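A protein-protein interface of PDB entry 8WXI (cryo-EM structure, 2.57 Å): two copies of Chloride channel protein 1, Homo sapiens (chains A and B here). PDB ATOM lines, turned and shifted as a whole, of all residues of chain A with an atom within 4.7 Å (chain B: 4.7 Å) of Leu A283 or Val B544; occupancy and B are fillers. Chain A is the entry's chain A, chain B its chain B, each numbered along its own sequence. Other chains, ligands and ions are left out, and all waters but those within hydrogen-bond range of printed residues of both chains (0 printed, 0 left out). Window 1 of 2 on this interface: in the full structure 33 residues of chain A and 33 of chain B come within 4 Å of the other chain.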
ATOM      1  N   THR A 281      19.162  29.515   8.085  1.00  0.00           N
ATOM      2  CA  THR A 281      18.752  28.534   9.095  1.00  0.00           C
ATOM      3  C   THR A 281      20.047  27.749   9.543  1.00  0.00           C
ATOM      4  O   THR A 281      20.286  26.663   9.039  1.00  0.00           O
ATOM      5  CB  THR A 281      17.473  27.749   8.863  1.00  0.00           C
ATOM      6  OG1 THR A 281      16.362  28.657   8.862  1.00  0.00           O
ATOM      7  CG2 THR A 281      17.256  26.789   9.934  1.00  0.00           C
ATOM      8  N   PRO A 282      20.927  28.339  10.434  1.00  0.00           N
ATOM      9  CA  PRO A 282      22.130  27.663  10.929  1.00  0.00           C
ATOM     10  C   PRO A 282      21.814  26.285  11.512  1.00  0.00           C
ATOM     11  O   PRO A 282      22.194  25.303  10.901  1.00  0.00           O
ATOM     12  CB  PRO A 282      22.622  28.598  12.027  1.00  0.00           C
ATOM     13  CG  PRO A 282      22.101  29.937  11.644  1.00  0.00           C
ATOM     14  CD  PRO A 282      20.775  29.694  10.987  1.00  0.00           C
ATOM     15  N   LEU A 283      21.127  26.214  12.650  1.00  0.00           N
ATOM     16  CA  LEU A 283      20.788  24.946  13.289  1.00  0.00           C
ATOM     17  C   LEU A 283      20.058  24.005  12.352  1.00  0.00           C
ATOM     18  O   LEU A 283      20.513  22.887  12.130  1.00  0.00           O
ATOM     19  CB  LEU A 283      19.938  25.180  14.535  1.00  0.00           C
ATOM     20  CG  LEU A 283      20.179  24.327  15.780  1.00  0.00           C
ATOM     21  CD1 LEU A 283      19.685  25.068  17.011  1.00  0.00           C
ATOM     22  CD2 LEU A 283      19.541  22.949  15.692  1.00  0.00           C
ATOM     23  N   GLY A 284      18.914  24.440  11.828  1.00  0.00           N
ATOM     24  CA  GLY A 284      18.151  23.596  10.933  1.00  0.00           C
ATOM     25  C   GLY A 284      18.979  23.085   9.786  1.00  0.00           C
ATOM     26  O   GLY A 284      18.840  21.937   9.418  1.00  0.00           O
ATOM     27  N   GLY A 285      19.839  23.924   9.218  1.00  0.00           N
ATOM     28  CA  GLY A 285      20.721  23.497   8.152  1.00  0.00           C
ATOM     29  C   GLY A 285      21.689  22.398   8.516  1.00  0.00           C
ATOM     30  O   GLY A 285      21.832  21.434   7.783  1.00  0.00           O
ATOM     31  N   VAL A 286      22.363  22.528   9.648  1.00  0.00           N
ATOM     32  CA  VAL A 286      23.255  21.467  10.095  1.00  0.00           C
ATOM     33  C   VAL A 286      22.461  20.195  10.314  1.00  0.00           C
ATOM     34  O   VAL A 286      22.818  19.150   9.801  1.00  0.00           O
ATOM     35  CB  VAL A 286      24.013  21.846  11.384  1.00  0.00           C
ATOM     36  CG1 VAL A 286      25.192  20.915  11.598  1.00  0.00           C
ATOM     37  CG2 VAL A 286      24.517  23.271  11.296  1.00  0.00           C
ATOM     38  N   LEU A 287      21.362  20.286  11.050  1.00  0.00           N
ATOM     39  CA  LEU A 287      20.522  19.122  11.302  1.00  0.00           C
ATOM     40  C   LEU A 287      20.072  18.481  10.002  1.00  0.00           C
ATOM     41  O   LEU A 287      20.127  17.263   9.863  1.00  0.00           O
ATOM     42  CB  LEU A 287      19.309  19.545  12.119  1.00  0.00           C
ATOM     43  CG  LEU A 287      19.307  19.308  13.627  1.00  0.00           C
ATOM     44  CD1 LEU A 287      18.271  18.255  13.986  1.00  0.00           C
ATOM     45  CD2 LEU A 287      20.680  18.908  14.142  1.00  0.00           C
ATOM     46  N   PHE A 306      28.161  23.578  12.522  1.00  0.00           N
ATOM     47  CA  PHE A 306      27.515  24.602  13.324  1.00  0.00           C
ATOM     48  C   PHE A 306      28.274  25.901  13.243  1.00  0.00           C
ATOM     49  O   PHE A 306      27.696  26.938  12.954  1.00  0.00           O
ATOM     50  CB  PHE A 306      27.471  24.159  14.778  1.00  0.00           C
ATOM     51  CG  PHE A 306      26.167  24.412  15.447  1.00  0.00           C
ATOM     52  CD1 PHE A 306      25.107  23.551  15.259  1.00  0.00           C
ATOM     53  CD2 PHE A 306      26.005  25.509  16.272  1.00  0.00           C
ATOM     54  CE1 PHE A 306      23.900  23.780  15.881  1.00  0.00           C
ATOM     55  CE2 PHE A 306      24.802  25.747  16.898  1.00  0.00           C
ATOM     56  CZ  PHE A 306      23.747  24.880  16.702  1.00  0.00           C
ATOM     57  N   VAL A 544      12.728  22.348  12.477  1.00  0.00           N
ATOM     58  CA  VAL A 544      13.683  23.344  12.957  1.00  0.00           C
ATOM     59  C   VAL A 544      13.942  24.415  11.913  1.00  0.00           C
ATOM     60  O   VAL A 544      14.038  25.592  12.243  1.00  0.00           O
ATOM     61  CB  VAL A 544      15.014  22.691  13.358  1.00  0.00           C
ATOM     62  CG1 VAL A 544      15.699  23.500  14.447  1.00  0.00           C
ATOM     63  CG2 VAL A 544      14.779  21.265  13.830  1.00  0.00           C
ATOM     64  N   GLU A 548      13.144  28.479  12.629  1.00  0.00           N
ATOM     65  CA  GLU A 548      14.082  29.568  12.440  1.00  0.00           C
ATOM     66  C   GLU A 548      13.691  30.509  11.317  1.00  0.00           C
ATOM     67  O   GLU A 548      13.867  31.712  11.446  1.00  0.00           O
ATOM     68  CB  GLU A 548      15.474  29.008  12.196  1.00  0.00           C
ATOM     69  CG  GLU A 548      16.266  28.762  13.465  1.00  0.00           C
ATOM     70  CD  GLU A 548      17.327  27.701  13.285  1.00  0.00           C
ATOM     71  OE1 GLU A 548      16.971  26.508  13.248  1.00  0.00           O
ATOM     72  OE2 GLU A 548      18.515  28.063  13.168  1.00  0.00           O
ATOM     73  N   THR B 281      12.094  19.974  26.495  1.00  0.00           N
ATOM     74  CA  THR B 281      12.915  20.413  25.361  1.00  0.00           C
ATOM     75  C   THR B 281      13.172  19.151  24.448  1.00  0.00           C
ATOM     76  O   THR B 281      14.221  18.537  24.566  1.00  0.00           O
ATOM     77  CB  THR B 281      14.071  21.360  25.631  1.00  0.00           C
ATOM     78  OG1 THR B 281      13.551  22.604  26.120  1.00  0.00           O
ATOM     79  CG2 THR B 281      14.803  21.640  24.405  1.00  0.00           C
ATOM     80  N   LEU B 283      13.627  18.660  20.881  1.00  0.00           N
ATOM     81  CA  LEU B 283      14.773  18.862  19.999  1.00  0.00           C
ATOM     82  C   LEU B 283      16.063  19.065  20.769  1.00  0.00           C
ATOM     83  O   LEU B 283      17.018  18.322  20.567  1.00  0.00           O
ATOM     84  CB  LEU B 283      14.541  20.057  19.078  1.00  0.00           C
ATOM     85  CG  LEU B 283      15.001  19.984  17.623  1.00  0.00           C
ATOM     86  CD1 LEU B 283      14.194  20.959  16.782  1.00  0.00           C
ATOM     87  CD2 LEU B 283      16.492  20.237  17.455  1.00  0.00           C
ATOM     88  N   GLY B 284      16.104  20.085  21.623  1.00  0.00           N
ATOM     89  CA  GLY B 284      17.304  20.351  22.387  1.00  0.00           C
ATOM     90  C   GLY B 284      17.781  19.141  23.143  1.00  0.00           C
ATOM     91  O   GLY B 284      18.970  18.904  23.196  1.00  0.00           O
ATOM     92  N   LEU B 287      19.423  16.629  20.672  1.00  0.00           N
ATOM     93  CA  LEU B 287      20.701  17.215  20.289  1.00  0.00           C
ATOM     94  C   LEU B 287      21.706  17.124  21.422  1.00  0.00           C
ATOM     95  O   LEU B 287      22.855  16.753  21.199  1.00  0.00           O
ATOM     96  CB  LEU B 287      20.490  18.671  19.899  1.00  0.00           C
ATOM     97  CG  LEU B 287      20.392  19.041  18.420  1.00  0.00           C
ATOM     98  CD1 LEU B 287      21.601  19.864  18.010  1.00  0.00           C
ATOM     99  CD2 LEU B 287      20.252  17.812  17.536  1.00  0.00           C
ATOM    100  N   VAL B 540      26.814  22.693  22.093  1.00  0.00           N
ATOM    101  CA  VAL B 540      26.208  23.880  21.519  1.00  0.00           C
ATOM    102  C   VAL B 540      24.703  23.704  21.459  1.00  0.00           C
ATOM    103  O   VAL B 540      23.993  24.573  20.966  1.00  0.00           O
ATOM    104  CB  VAL B 540      26.757  24.164  20.113  1.00  0.00           C
ATOM    105  CG1 VAL B 540      28.024  25.003  20.197  1.00  0.00           C
ATOM    106  CG2 VAL B 540      27.024  22.863  19.375  1.00  0.00           C
ATOM    107  N   SER B 541      24.208  22.589  21.982  1.00  0.00           N
ATOM    108  CA  SER B 541      22.780  22.300  21.940  1.00  0.00           C
ATOM    109  C   SER B 541      22.045  22.976  23.058  1.00  0.00           C
ATOM    110  O   SER B 541      20.827  22.917  23.121  1.00  0.00           O
ATOM    111  CB  SER B 541      22.568  20.812  22.069  1.00  0.00           C
ATOM    112  OG  SER B 541      23.578  20.248  22.876  1.00  0.00           O
ATOM    113  N   THR B 542      22.777  23.625  23.946  1.00  0.00           N
ATOM    114  CA  THR B 542      22.169  24.341  25.045  1.00  0.00           C
ATOM    115  C   THR B 542      21.478  25.561  24.504  1.00  0.00           C
ATOM    116  O   THR B 542      20.562  26.070  25.124  1.00  0.00           O
ATOM    117  CB  THR B 542      23.236  24.758  26.041  1.00  0.00           C
ATOM    118  OG1 THR B 542      24.244  25.512  25.361  1.00  0.00           O
ATOM    119  CG2 THR B 542      23.869  23.532  26.632  1.00  0.00           C
ATOM    120  N   ALA B 543      21.919  26.042  23.348  1.00  0.00           N
ATOM    121  CA  ALA B 543      21.263  27.162  22.708  1.00  0.00           C
ATOM    122  C   ALA B 543      19.867  26.734  22.333  1.00  0.00           C
ATOM    123  O   ALA B 543      18.919  27.455  22.590  1.00  0.00           O
ATOM    124  CB  ALA B 543      22.038  27.579  21.477  1.00  0.00           C
ATOM    125  N   VAL B 544      19.733  25.551  21.741  1.00  0.00           N
ATOM    126  CA  VAL B 544      18.423  25.024  21.368  1.00  0.00           C
ATOM    127  C   VAL B 544      17.570  24.737  22.590  1.00  0.00           C
ATOM    128  O   VAL B 544      16.374  25.011  22.590  1.00  0.00           O
ATOM    129  CB  VAL B 544      18.556  23.745  20.528  1.00  0.00           C
ATOM    130  CG1 VAL B 544      17.370  23.597  19.589  1.00  0.00           C
ATOM    131  CG2 VAL B 544      19.854  23.768  19.737  1.00  0.00           C
ATOM    132  N   ILE B 545      18.175  24.191  23.637  1.00  0.00           N
ATOM    133  CA  ILE B 545      17.443  23.952  24.869  1.00  0.00           C
ATOM    134  C   ILE B 545      16.886  25.271  25.358  1.00  0.00           C
ATOM    135  O   ILE B 545      15.706  25.369  25.662  1.00  0.00           O
ATOM    136  CB  ILE B 545      18.328  23.290  25.940  1.00  0.00           C
ATOM    137  CG1 ILE B 545      18.695  21.872  25.522  1.00  0.00           C
ATOM    138  CG2 ILE B 545      17.626  23.246  27.289  1.00  0.00           C
ATOM    139  CD1 ILE B 545      19.725  21.220  26.409  1.00  0.00           C
ATOM    140  N   CYS B 546      17.722  26.298  25.393  1.00  0.00           N
ATOM    141  CA  CYS B 546      17.282  27.614  25.824  1.00  0.00           C
ATOM    142  C   CYS B 546      16.144  28.120  24.972  1.00  0.00           C
ATOM    143  O   CYS B 546      15.146  28.547  25.502  1.00  0.00           O
ATOM    144  CB  CYS B 546      18.433  28.607  25.774  1.00  0.00           C
ATOM    145  SG  CYS B 546      18.986  29.176  27.384  1.00  0.00           S
ATOM    146  N   PHE B 547      16.290  28.069  23.655  1.00  0.00           N
ATOM    147  CA  PHE B 547      15.247  28.538  22.751  1.00  0.00           C
ATOM    148  C   PHE B 547      13.907  27.934  23.086  1.00  0.00           C
ATOM    149  O   PHE B 547      12.922  28.643  23.207  1.00  0.00           O
ATOM    150  CB  PHE B 547      15.573  28.166  21.314  1.00  0.00           C
ATOM    151  CG  PHE B 547      16.680  28.968  20.716  1.00  0.00           C
ATOM    152  CD1 PHE B 547      16.849  30.298  21.046  1.00  0.00           C
ATOM    153  CD2 PHE B 547      17.545  28.389  19.808  1.00  0.00           C
ATOM    154  CE1 PHE B 547      17.867  31.035  20.484  1.00  0.00           C
ATOM    155  CE2 PHE B 547      18.573  29.115  19.253  1.00  0.00           C
ATOM    156  CZ  PHE B 547      18.735  30.438  19.597  1.00  0.00           C
ATOM    157  N   GLU B 548      13.864  26.616  23.225  1.00  0.00           N
ATOM    158  CA  GLU B 548      12.613  25.939  23.508  1.00  0.00           C
ATOM    159  C   GLU B 548      12.089  26.206  24.906  1.00  0.00           C
ATOM    160  O   GLU B 548      10.889  26.355  25.084  1.00  0.00           O
ATOM    161  CB  GLU B 548      12.779  24.445  23.285  1.00  0.00           C
ATOM    162  CG  GLU B 548      12.506  24.005  21.860  1.00  0.00           C
ATOM    163  CD  GLU B 548      13.222  22.721  21.507  1.00  0.00           C
ATOM    164  OE1 GLU B 548      14.447  22.768  21.283  1.00  0.00           O
ATOM    165  OE2 GLU B 548      12.561  21.665  21.466  1.00  0.00           O
ATOM    166  N   MET B 560      23.890  31.692  19.117  1.00  0.00           N
ATOM    167  CA  MET B 560      24.800  30.809  18.417  1.00  0.00           C
ATOM    168  C   MET B 560      26.223  31.284  18.566  1.00  0.00           C
ATOM    169  O   MET B 560      27.076  30.525  18.992  1.00  0.00           O
ATOM    170  CB  MET B 560      24.430  30.729  16.945  1.00  0.00           C
ATOM    171  CG  MET B 560      24.126  29.324  16.467  1.00  0.00           C
ATOM    172  SD  MET B 560      22.379  29.104  16.101  1.00  0.00           S
ATOM    173  CE  MET B 560      21.845  28.179  17.537  1.00  0.00           C
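Leu A283 touches Val B544, and with the chains exchanged Val A544 touches Leu B283. Leu A287 touches its own counterpart, Leu B287. Positions printed for both chains: 281, 283, 284, 287, 544 and 548. Of the 5 pairs that touch across the chains among the printed residues, 3 have their exchanged pair printed and touching as well.
N of Leu A283 lies within hydrogen-bond range of OE2 of Glu A548. OE2 of Glu B548 is in hydrogen-bond range of N of Leu B283.
Of the printed residues of chain B, Leu A283 touches Val B544 (3.0 Å) and Met B560 (3.8 Å). Printed residues of chain B within 4 Å of Val A544: Leu B283 (3.0 Å). Printed residues of chain A within 4 Å of Leu B283: Val A544. Of the printed residues of chain A, Leu B287 touches Leu A287. Of the printed residues of chain A, Val B544 touches Leu A283 (3.0 Å). Cys B546 touches none of the printed residues of chain A. The nearest residue of chain B that does not touch Leu A283 is Leu B287 (4.4 Å). The nearest printed residue of chain A that does not touch Val B544 is Phe A306 (5.1 Å).
CG2 of Val B544 touches CD1 of Leu A283 (3.0 Å). Leu A283 touches Met B560 (CD1 to CE, 3.8 Å). Leu A287 touches Leu B287 (CD2 to CD2, 3.6 Å). Phe A306 touches Met B560 (CE2 to CG, 3.7 Å). Leu B283 touches Val A544.
Along chain B the printed residues that touch a printed residue of chain A span positions 283 to 560. Among the printed residues, 5 pairs touch across the chains. Among the printed residues, no Asp or Glu carboxylate lies within 4 Å of a Lys or Arg side-chain nitrogen of the other chain.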
